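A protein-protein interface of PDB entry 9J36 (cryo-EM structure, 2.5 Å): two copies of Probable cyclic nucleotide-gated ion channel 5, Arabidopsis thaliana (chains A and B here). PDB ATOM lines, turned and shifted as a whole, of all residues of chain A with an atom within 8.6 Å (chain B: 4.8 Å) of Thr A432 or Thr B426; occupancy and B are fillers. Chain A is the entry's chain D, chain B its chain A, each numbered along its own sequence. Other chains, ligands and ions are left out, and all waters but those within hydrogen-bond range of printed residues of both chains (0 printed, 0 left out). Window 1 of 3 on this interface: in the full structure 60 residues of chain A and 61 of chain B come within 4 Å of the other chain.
O of Gly B422 lies within hydrogen-bond range of OG1 of Thr B426, 2.5 Å away. O of Leu A428 sits at hydrogen-bond distance from OG1 of Thr A432. OE2 of Glu A436 lies within salt-bridge range of NH1 of Arg A439.
Among the printed residues, pairs that only touch across the chains: Leu A431 with Arg B259, Val A440 with Ser B430, Leu A435 with Arg B259, Leu A428 with Asn B423, Leu A435 with Lys B258, Gln A425 with Gln B425, Thr A432 with Lys B258, Thr A432 with Thr B426 and Thr A432 with Arg B259.
Of the 19 printed residues of chain A, 9 touch a printed residue of chain B.
Gln B425 touches its own counterpart, Gln A425. Gln A425 touches Thr B426, but with the chains exchanged Thr A426 does not touch Gln B425 (7.5 Å). Gln A429 touches its own counterpart, Gln B429. 7 positions are printed for both chains. Of the 14 pairs that touch across the chains among the printed residues, 2 have their exchanged pair printed and touching as well.
Tyr A427 touches none of the printed residues of chain B. Printed residues of chain B within 4 Å of Leu A428: Asn B423 (3.4 Å). Printed residues of chain B within 4 Å of Gln A429: Gln B429. Of the printed residues of chain B, Thr A432 touches Lys B258, Arg B259 and Thr B426. Printed residues of chain A within 4 Å of Arg B259: Leu A431, Thr A432 and Leu A435. Of the printed residues of chain A, Asn B423 touches Leu A428 (3.4 Å). Met B424 touches none of the printed residues of chain A. Thr B426 touches two residues of chain A. Of the printed residues of chain A, Gln B429 touches Gln A429.
O of Gly B422 sits close to OE1 of Gln A425, at 2.7 Å. OG1 of Thr B426 is in hydrogen-bond range of OE1 of Gln A425 (2.9 Å). The side-chain amide oxygen (OE1) of Gln B429 is in hydrogen-bond range of the side-chain amide nitrogen (NE2) of Gln A429, at 3.3 Å. The side-chain carboxylate (OE1) of Glu A436 sits at hydrogen-bond distance from the side-chain hydroxyl (OG) of Ser B430, at 3.2 Å. The side-chain hydroxyl (OG) of Ser B430 lies within hydrogen-bond range of the guanidinium group (NH2) of Arg A443 (3.1 Å).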
ATOM      1  N   MET A 424      -5.253  27.320   8.539  1.00  0.00           N
ATOM      2  CA  MET A 424      -6.129  26.240   8.954  1.00  0.00           C
ATOM      3  C   MET A 424      -5.389  24.933   9.150  1.00  0.00           C
ATOM      4  O   MET A 424      -5.681  24.211  10.103  1.00  0.00           O
ATOM      5  CB  MET A 424      -7.250  26.044   7.931  1.00  0.00           C
ATOM      6  CG  MET A 424      -8.377  25.169   8.419  1.00  0.00           C
ATOM      7  SD  MET A 424      -9.639  26.102   9.294  1.00  0.00           S
ATOM      8  CE  MET A 424     -10.271  27.140   7.983  1.00  0.00           C
ATOM      9  N   GLN A 425      -4.431  24.622   8.276  1.00  0.00           N
ATOM     10  CA  GLN A 425      -3.574  23.460   8.471  1.00  0.00           C
ATOM     11  C   GLN A 425      -2.700  23.608   9.706  1.00  0.00           C
ATOM     12  O   GLN A 425      -2.509  22.633  10.431  1.00  0.00           O
ATOM     13  CB  GLN A 425      -2.756  23.228   7.198  1.00  0.00           C
ATOM     14  CG  GLN A 425      -1.395  22.543   7.307  1.00  0.00           C
ATOM     15  CD  GLN A 425      -1.388  21.175   7.951  1.00  0.00           C
ATOM     16  OE1 GLN A 425      -2.334  20.421   7.834  1.00  0.00           O
ATOM     17  NE2 GLN A 425      -0.286  20.837   8.604  1.00  0.00           N
ATOM     18  N   THR A 426      -2.191  24.807   9.980  1.00  0.00           N
ATOM     19  CA  THR A 426      -1.417  25.048  11.192  1.00  0.00           C
ATOM     20  C   THR A 426      -2.247  24.882  12.457  1.00  0.00           C
ATOM     21  O   THR A 426      -1.742  24.352  13.446  1.00  0.00           O
ATOM     22  CB  THR A 426      -0.806  26.446  11.136  1.00  0.00           C
ATOM     23  OG1 THR A 426      -0.137  26.613   9.885  1.00  0.00           O
ATOM     24  CG2 THR A 426       0.194  26.657  12.233  1.00  0.00           C
ATOM     25  N   TYR A 427      -3.510  25.284  12.438  1.00  0.00           N
ATOM     26  CA  TYR A 427      -4.411  25.046  13.552  1.00  0.00           C
ATOM     27  C   TYR A 427      -4.757  23.578  13.729  1.00  0.00           C
ATOM     28  O   TYR A 427      -4.694  23.074  14.852  1.00  0.00           O
ATOM     29  CB  TYR A 427      -5.702  25.853  13.367  1.00  0.00           C
ATOM     30  CG  TYR A 427      -6.762  25.563  14.402  1.00  0.00           C
ATOM     31  CD1 TYR A 427      -6.665  26.086  15.681  1.00  0.00           C
ATOM     32  CD2 TYR A 427      -7.862  24.770  14.100  1.00  0.00           C
ATOM     33  CE1 TYR A 427      -7.621  25.821  16.628  1.00  0.00           C
ATOM     34  CE2 TYR A 427      -8.812  24.493  15.041  1.00  0.00           C
ATOM     35  CZ  TYR A 427      -8.689  25.020  16.302  1.00  0.00           C
ATOM     36  OH  TYR A 427      -9.653  24.754  17.242  1.00  0.00           O
ATOM     37  N   LEU A 428      -5.139  22.888  12.655  1.00  0.00           N
ATOM     38  CA  LEU A 428      -5.531  21.489  12.724  1.00  0.00           C
ATOM     39  C   LEU A 428      -4.384  20.557  13.055  1.00  0.00           C
ATOM     40  O   LEU A 428      -4.604  19.541  13.716  1.00  0.00           O
ATOM     41  CB  LEU A 428      -6.136  21.037  11.397  1.00  0.00           C
ATOM     42  CG  LEU A 428      -7.518  21.552  11.033  1.00  0.00           C
ATOM     43  CD1 LEU A 428      -7.734  21.359   9.554  1.00  0.00           C
ATOM     44  CD2 LEU A 428      -8.568  20.821  11.835  1.00  0.00           C
ATOM     45  N   GLN A 429      -3.179  20.867  12.595  1.00  0.00           N
ATOM     46  CA  GLN A 429      -2.006  20.072  12.894  1.00  0.00           C
ATOM     47  C   GLN A 429      -1.598  20.185  14.348  1.00  0.00           C
ATOM     48  O   GLN A 429      -1.183  19.190  14.942  1.00  0.00           O
ATOM     49  CB  GLN A 429      -0.869  20.520  11.983  1.00  0.00           C
ATOM     50  CG  GLN A 429       0.380  19.712  12.056  1.00  0.00           C
ATOM     51  CD  GLN A 429       1.586  20.545  11.738  1.00  0.00           C
ATOM     52  OE1 GLN A 429       1.490  21.765  11.620  1.00  0.00           O
ATOM     53  NE2 GLN A 429       2.734  19.900  11.596  1.00  0.00           N
ATOM     54  N   SER A 430      -1.720  21.362  14.932  1.00  0.00           N
ATOM     55  CA  SER A 430      -1.488  21.563  16.349  1.00  0.00           C
ATOM     56  C   SER A 430      -2.608  21.026  17.214  1.00  0.00           C
ATOM     57  O   SER A 430      -2.410  20.834  18.412  1.00  0.00           O
ATOM     58  CB  SER A 430      -1.306  23.047  16.627  1.00  0.00           C
ATOM     59  OG  SER A 430      -1.414  23.317  18.003  1.00  0.00           O
ATOM     60  N   LEU A 431      -3.780  20.798  16.644  1.00  0.00           N
ATOM     61  CA  LEU A 431      -4.902  20.255  17.381  1.00  0.00           C
ATOM     62  C   LEU A 431      -4.792  18.762  17.617  1.00  0.00           C
ATOM     63  O   LEU A 431      -5.038  18.309  18.734  1.00  0.00           O
ATOM     64  CB  LEU A 431      -6.199  20.550  16.634  1.00  0.00           C
ATOM     65  CG  LEU A 431      -7.474  20.616  17.452  1.00  0.00           C
ATOM     66  CD1 LEU A 431      -7.573  21.960  18.116  1.00  0.00           C
ATOM     67  CD2 LEU A 431      -8.645  20.370  16.543  1.00  0.00           C
ATOM     68  N   THR A 432      -4.406  17.997  16.610  1.00  0.00           N
ATOM     69  CA  THR A 432      -4.320  16.547  16.684  1.00  0.00           C
ATOM     70  C   THR A 432      -2.875  16.087  16.791  1.00  0.00           C
ATOM     71  O   THR A 432      -2.481  15.100  16.184  1.00  0.00           O
ATOM     72  CB  THR A 432      -4.983  15.903  15.472  1.00  0.00           C
ATOM     73  OG1 THR A 432      -4.321  16.339  14.282  1.00  0.00           O
ATOM     74  CG2 THR A 432      -6.438  16.289  15.393  1.00  0.00           C
ATOM     75  N   ILE A 433      -2.060  16.806  17.559  1.00  0.00           N
ATOM     76  CA  ILE A 433      -0.632  16.519  17.607  1.00  0.00           C
ATOM     77  C   ILE A 433      -0.346  15.257  18.418  1.00  0.00           C
ATOM     78  O   ILE A 433       0.483  14.432  18.023  1.00  0.00           O
ATOM     79  CB  ILE A 433       0.119  17.756  18.139  1.00  0.00           C
ATOM     80  CG1 ILE A 433       1.600  17.473  18.321  1.00  0.00           C
ATOM     81  CG2 ILE A 433      -0.485  18.261  19.421  1.00  0.00           C
ATOM     82  CD1 ILE A 433       2.380  18.668  18.648  1.00  0.00           C
ATOM     83  N   ARG A 434      -1.057  15.049  19.523  1.00  0.00           N
ATOM     84  CA  ARG A 434      -0.870  13.876  20.355  1.00  0.00           C
ATOM     85  C   ARG A 434      -1.420  12.618  19.723  1.00  0.00           C
ATOM     86  O   ARG A 434      -0.825  11.552  19.884  1.00  0.00           O
ATOM     87  CB  ARG A 434      -1.535  14.077  21.711  1.00  0.00           C
ATOM     88  CG  ARG A 434      -1.019  15.241  22.472  1.00  0.00           C
ATOM     89  CD  ARG A 434       0.307  14.928  23.055  1.00  0.00           C
ATOM     90  NE  ARG A 434       0.915  16.098  23.658  1.00  0.00           N
ATOM     91  CZ  ARG A 434       2.009  16.679  23.197  1.00  0.00           C
ATOM     92  NH1 ARG A 434       2.611  16.198  22.126  1.00  0.00           N
ATOM     93  NH2 ARG A 434       2.497  17.744  23.804  1.00  0.00           N
ATOM     94  N   LEU A 435      -2.524  12.721  18.999  1.00  0.00           N
ATOM     95  CA  LEU A 435      -3.061  11.606  18.246  1.00  0.00           C
ATOM     96  C   LEU A 435      -2.159  11.183  17.106  1.00  0.00           C
ATOM     97  O   LEU A 435      -1.949   9.983  16.918  1.00  0.00           O
ATOM     98  CB  LEU A 435      -4.441  11.963  17.697  1.00  0.00           C
ATOM     99  CG  LEU A 435      -5.204  10.889  16.932  1.00  0.00           C
ATOM    100  CD1 LEU A 435      -5.918   9.969  17.867  1.00  0.00           C
ATOM    101  CD2 LEU A 435      -6.168  11.528  15.984  1.00  0.00           C
ATOM    102  N   GLU A 436      -1.613  12.130  16.354  1.00  0.00           N
ATOM    103  CA  GLU A 436      -0.659  11.788  15.317  1.00  0.00           C
ATOM    104  C   GLU A 436       0.641  11.240  15.881  1.00  0.00           C
ATOM    105  O   GLU A 436       1.231  10.354  15.267  1.00  0.00           O
ATOM    106  CB  GLU A 436      -0.373  12.999  14.436  1.00  0.00           C
ATOM    107  CG  GLU A 436      -1.523  13.441  13.539  1.00  0.00           C
ATOM    108  CD  GLU A 436      -2.321  12.300  12.930  1.00  0.00           C
ATOM    109  OE1 GLU A 436      -1.761  11.503  12.156  1.00  0.00           O
ATOM    110  OE2 GLU A 436      -3.531  12.208  13.211  1.00  0.00           O
ATOM    111  N   GLU A 437       1.084  11.718  17.040  1.00  0.00           N
ATOM    112  CA  GLU A 437       2.207  11.114  17.740  1.00  0.00           C
ATOM    113  C   GLU A 437       1.935   9.689  18.178  1.00  0.00           C
ATOM    114  O   GLU A 437       2.825   8.845  18.059  1.00  0.00           O
ATOM    115  CB  GLU A 437       2.578  11.937  18.964  1.00  0.00           C
ATOM    116  CG  GLU A 437       3.429  13.129  18.658  1.00  0.00           C
ATOM    117  CD  GLU A 437       3.743  13.934  19.887  1.00  0.00           C
ATOM    118  OE1 GLU A 437       3.355  13.500  20.991  1.00  0.00           O
ATOM    119  OE2 GLU A 437       4.375  14.998  19.751  1.00  0.00           O
ATOM    120  N   MET A 438       0.736   9.406  18.669  1.00  0.00           N
ATOM    121  CA  MET A 438       0.324   8.049  18.987  1.00  0.00           C
ATOM    122  C   MET A 438       0.286   7.155  17.763  1.00  0.00           C
ATOM    123  O   MET A 438       0.658   5.988  17.851  1.00  0.00           O
ATOM    124  CB  MET A 438      -1.055   8.061  19.645  1.00  0.00           C
ATOM    125  CG  MET A 438      -1.440   6.776  20.344  1.00  0.00           C
ATOM    126  SD  MET A 438      -2.441   5.681  19.330  1.00  0.00           S
ATOM    127  CE  MET A 438      -3.656   6.819  18.698  1.00  0.00           C
ATOM    128  N   ARG A 439      -0.133   7.680  16.621  1.00  0.00           N
ATOM    129  CA  ARG A 439      -0.178   6.875  15.411  1.00  0.00           C
ATOM    130  C   ARG A 439       1.204   6.620  14.830  1.00  0.00           C
ATOM    131  O   ARG A 439       1.448   5.536  14.295  1.00  0.00           O
ATOM    132  CB  ARG A 439      -1.077   7.546  14.386  1.00  0.00           C
ATOM    133  CG  ARG A 439      -2.511   7.538  14.826  1.00  0.00           C
ATOM    134  CD  ARG A 439      -3.357   8.462  14.011  1.00  0.00           C
ATOM    135  NE  ARG A 439      -4.770   8.240  14.281  1.00  0.00           N
ATOM    136  CZ  ARG A 439      -5.750   8.783  13.575  1.00  0.00           C
ATOM    137  NH1 ARG A 439      -5.463   9.580  12.558  1.00  0.00           N
ATOM    138  NH2 ARG A 439      -7.012   8.526  13.886  1.00  0.00           N
ATOM    139  N   VAL A 440       2.116   7.584  14.946  1.00  0.00           N
ATOM    140  CA  VAL A 440       3.505   7.362  14.561  1.00  0.00           C
ATOM    141  C   VAL A 440       4.151   6.325  15.468  1.00  0.00           C
ATOM    142  O   VAL A 440       4.830   5.408  14.994  1.00  0.00           O
ATOM    143  CB  VAL A 440       4.274   8.693  14.583  1.00  0.00           C
ATOM    144  CG1 VAL A 440       5.747   8.470  14.450  1.00  0.00           C
ATOM    145  CG2 VAL A 440       3.810   9.566  13.479  1.00  0.00           C
ATOM    146  N   ARG A 443       2.696   2.891  14.520  1.00  0.00           N
ATOM    147  CA  ARG A 443       3.320   2.355  13.320  1.00  0.00           C
ATOM    148  C   ARG A 443       4.753   1.902  13.539  1.00  0.00           C
ATOM    149  O   ARG A 443       5.160   0.889  12.961  1.00  0.00           O
ATOM    150  CB  ARG A 443       3.290   3.398  12.206  1.00  0.00           C
ATOM    151  CG  ARG A 443       1.974   3.469  11.498  1.00  0.00           C
ATOM    152  CD  ARG A 443       2.015   4.401  10.320  1.00  0.00           C
ATOM    153  NE  ARG A 443       1.848   5.793  10.707  1.00  0.00           N
ATOM    154  CZ  ARG A 443       0.695   6.445  10.621  1.00  0.00           C
ATOM    155  NH1 ARG A 443      -0.381   5.827  10.168  1.00  0.00           N
ATOM    156  NH2 ARG A 443       0.613   7.713  10.985  1.00  0.00           N
ATOM    157  N   TRP A 470      -2.488   5.216  25.917  1.00  0.00           N
ATOM    158  CA  TRP A 470      -3.121   6.289  25.172  1.00  0.00           C
ATOM    159  C   TRP A 470      -4.491   6.640  25.730  1.00  0.00           C
ATOM    160  O   TRP A 470      -4.864   7.813  25.735  1.00  0.00           O
ATOM    161  CB  TRP A 470      -3.238   5.907  23.703  1.00  0.00           C
ATOM    162  CG  TRP A 470      -4.153   6.782  22.939  1.00  0.00           C
ATOM    163  CD1 TRP A 470      -5.369   6.451  22.450  1.00  0.00           C
ATOM    164  CD2 TRP A 470      -3.935   8.148  22.586  1.00  0.00           C
ATOM    165  NE1 TRP A 470      -5.926   7.519  21.808  1.00  0.00           N
ATOM    166  CE2 TRP A 470      -5.061   8.575  21.878  1.00  0.00           C
ATOM    167  CE3 TRP A 470      -2.893   9.049  22.794  1.00  0.00           C
ATOM    168  CZ2 TRP A 470      -5.178   9.858  21.381  1.00  0.00           C
ATOM    169  CZ3 TRP A 470      -3.013  10.313  22.296  1.00  0.00           C
ATOM    170  CH2 TRP A 470      -4.146  10.711  21.605  1.00  0.00           C
ATOM    171  N   LYS B 258     -12.242  13.580  17.130  1.00  0.00           N
ATOM    172  CA  LYS B 258     -11.244  13.582  16.069  1.00  0.00           C
ATOM    173  C   LYS B 258      -9.896  14.014  16.622  1.00  0.00           C
ATOM    174  O   LYS B 258      -8.851  13.617  16.099  1.00  0.00           O
ATOM    175  CB  LYS B 258     -11.669  14.491  14.909  1.00  0.00           C
ATOM    176  CG  LYS B 258     -12.716  13.872  14.002  1.00  0.00           C
ATOM    177  CD  LYS B 258     -12.299  12.475  13.576  1.00  0.00           C
ATOM    178  CE  LYS B 258     -13.478  11.672  13.084  1.00  0.00           C
ATOM    179  NZ  LYS B 258     -13.090  10.273  12.800  1.00  0.00           N
ATOM    180  N   ARG B 259      -9.907  14.837  17.675  1.00  0.00           N
ATOM    181  CA  ARG B 259      -8.666  15.206  18.347  1.00  0.00           C
ATOM    182  C   ARG B 259      -8.075  14.054  19.144  1.00  0.00           C
ATOM    183  O   ARG B 259      -6.868  13.814  19.053  1.00  0.00           O
ATOM    184  CB  ARG B 259      -8.891  16.407  19.270  1.00  0.00           C
ATOM    185  CG  ARG B 259      -7.623  16.855  19.965  1.00  0.00           C
ATOM    186  CD  ARG B 259      -7.762  18.128  20.780  1.00  0.00           C
ATOM    187  NE  ARG B 259      -8.067  17.879  22.184  1.00  0.00           N
ATOM    188  CZ  ARG B 259      -7.194  18.046  23.172  1.00  0.00           C
ATOM    189  NH1 ARG B 259      -5.959  18.435  22.903  1.00  0.00           N
ATOM    190  NH2 ARG B 259      -7.548  17.811  24.429  1.00  0.00           N
ATOM    191  N   GLY B 422      -6.223  20.360   4.988  1.00  0.00           N
ATOM    192  CA  GLY B 422      -5.468  20.399   6.209  1.00  0.00           C
ATOM    193  C   GLY B 422      -5.509  19.119   6.990  1.00  0.00           C
ATOM    194  O   GLY B 422      -4.563  18.823   7.715  1.00  0.00           O
ATOM    195  N   ASN B 423      -6.567  18.337   6.878  1.00  0.00           N
ATOM    196  CA  ASN B 423      -6.564  17.043   7.533  1.00  0.00           C
ATOM    197  C   ASN B 423      -5.943  15.966   6.672  1.00  0.00           C
ATOM    198  O   ASN B 423      -5.567  14.918   7.201  1.00  0.00           O
ATOM    199  CB  ASN B 423      -7.979  16.641   7.931  1.00  0.00           C
ATOM    200  CG  ASN B 423      -8.275  16.966   9.367  1.00  0.00           C
ATOM    201  OD1 ASN B 423      -8.001  16.173  10.264  1.00  0.00           O
ATOM    202  ND2 ASN B 423      -8.832  18.143   9.599  1.00  0.00           N
ATOM    203  N   MET B 424      -5.821  16.185   5.371  1.00  0.00           N
ATOM    204  CA  MET B 424      -5.095  15.266   4.515  1.00  0.00           C
ATOM    205  C   MET B 424      -3.595  15.473   4.578  1.00  0.00           C
ATOM    206  O   MET B 424      -2.850  14.493   4.592  1.00  0.00           O
ATOM    207  CB  MET B 424      -5.569  15.401   3.067  1.00  0.00           C
ATOM    208  CG  MET B 424      -5.106  14.286   2.164  1.00  0.00           C
ATOM    209  SD  MET B 424      -6.233  12.887   2.170  1.00  0.00           S
ATOM    210  CE  MET B 424      -7.694  13.619   1.443  1.00  0.00           C
ATOM    211  N   GLN B 425      -3.141  16.725   4.630  1.00  0.00           N
ATOM    212  CA  GLN B 425      -1.728  17.012   4.837  1.00  0.00           C
ATOM    213  C   GLN B 425      -1.258  16.556   6.209  1.00  0.00           C
ATOM    214  O   GLN B 425      -0.152  16.032   6.326  1.00  0.00           O
ATOM    215  CB  GLN B 425      -1.484  18.504   4.600  1.00  0.00           C
ATOM    216  CG  GLN B 425      -0.326  19.190   5.324  1.00  0.00           C
ATOM    217  CD  GLN B 425       1.045  18.598   5.095  1.00  0.00           C
ATOM    218  OE1 GLN B 425       1.336  18.082   4.034  1.00  0.00           O
ATOM    219  NE2 GLN B 425       1.913  18.714   6.090  1.00  0.00           N
ATOM    220  N   THR B 426      -2.081  16.712   7.243  1.00  0.00           N
ATOM    221  CA  THR B 426      -1.739  16.221   8.572  1.00  0.00           C
ATOM    222  C   THR B 426      -1.631  14.703   8.624  1.00  0.00           C
ATOM    223  O   THR B 426      -0.746  14.181   9.303  1.00  0.00           O
ATOM    224  CB  THR B 426      -2.774  16.715   9.581  1.00  0.00           C
ATOM    225  OG1 THR B 426      -2.942  18.124   9.425  1.00  0.00           O
ATOM    226  CG2 THR B 426      -2.344  16.447  10.992  1.00  0.00           C
ATOM    227  N   TYR B 427      -2.478  13.987   7.897  1.00  0.00           N
ATOM    228  CA  TYR B 427      -2.365  12.544   7.781  1.00  0.00           C
ATOM    229  C   TYR B 427      -1.138  12.109   6.998  1.00  0.00           C
ATOM    230  O   TYR B 427      -0.417  11.217   7.452  1.00  0.00           O
ATOM    231  CB  TYR B 427      -3.622  11.969   7.118  1.00  0.00           C
ATOM    232  CG  TYR B 427      -3.539  10.490   6.823  1.00  0.00           C
ATOM    233  CD1 TYR B 427      -3.694   9.557   7.836  1.00  0.00           C
ATOM    234  CD2 TYR B 427      -3.313  10.027   5.534  1.00  0.00           C
ATOM    235  CE1 TYR B 427      -3.614   8.212   7.576  1.00  0.00           C
ATOM    236  CE2 TYR B 427      -3.221   8.690   5.269  1.00  0.00           C
ATOM    237  CZ  TYR B 427      -3.373   7.786   6.292  1.00  0.00           C
ATOM    238  OH  TYR B 427      -3.296   6.443   6.022  1.00  0.00           O
ATOM    239  N   LEU B 428      -0.899  12.697   5.827  1.00  0.00           N
ATOM    240  CA  LEU B 428       0.224  12.324   4.980  1.00  0.00           C
ATOM    241  C   LEU B 428       1.570  12.690   5.569  1.00  0.00           C
ATOM    242  O   LEU B 428       2.543  11.969   5.342  1.00  0.00           O
ATOM    243  CB  LEU B 428       0.110  12.997   3.615  1.00  0.00           C
ATOM    244  CG  LEU B 428      -0.958  12.493   2.659  1.00  0.00           C
ATOM    245  CD1 LEU B 428      -1.189  13.535   1.597  1.00  0.00           C
ATOM    246  CD2 LEU B 428      -0.527  11.179   2.050  1.00  0.00           C
ATOM    247  N   GLN B 429       1.651  13.796   6.296  1.00  0.00           N
ATOM    248  CA  GLN B 429       2.878  14.211   6.945  1.00  0.00           C
ATOM    249  C   GLN B 429       3.250  13.299   8.096  1.00  0.00           C
ATOM    250  O   GLN B 429       4.430  13.013   8.288  1.00  0.00           O
ATOM    251  CB  GLN B 429       2.711  15.645   7.433  1.00  0.00           C
ATOM    252  CG  GLN B 429       3.929  16.285   8.002  1.00  0.00           C
ATOM    253  CD  GLN B 429       3.571  17.309   9.038  1.00  0.00           C
ATOM    254  OE1 GLN B 429       2.413  17.420   9.434  1.00  0.00           O
ATOM    255  NE2 GLN B 429       4.556  18.070   9.486  1.00  0.00           N
ATOM    256  N   SER B 430       2.272  12.828   8.849  1.00  0.00           N
ATOM    257  CA  SER B 430       2.488  11.847   9.893  1.00  0.00           C
ATOM    258  C   SER B 430       2.733  10.453   9.353  1.00  0.00           C
ATOM    259  O   SER B 430       3.242   9.603  10.081  1.00  0.00           O
ATOM    260  CB  SER B 430       1.285  11.821  10.823  1.00  0.00           C
ATOM    261  OG  SER B 430       1.302  10.673  11.634  1.00  0.00           O
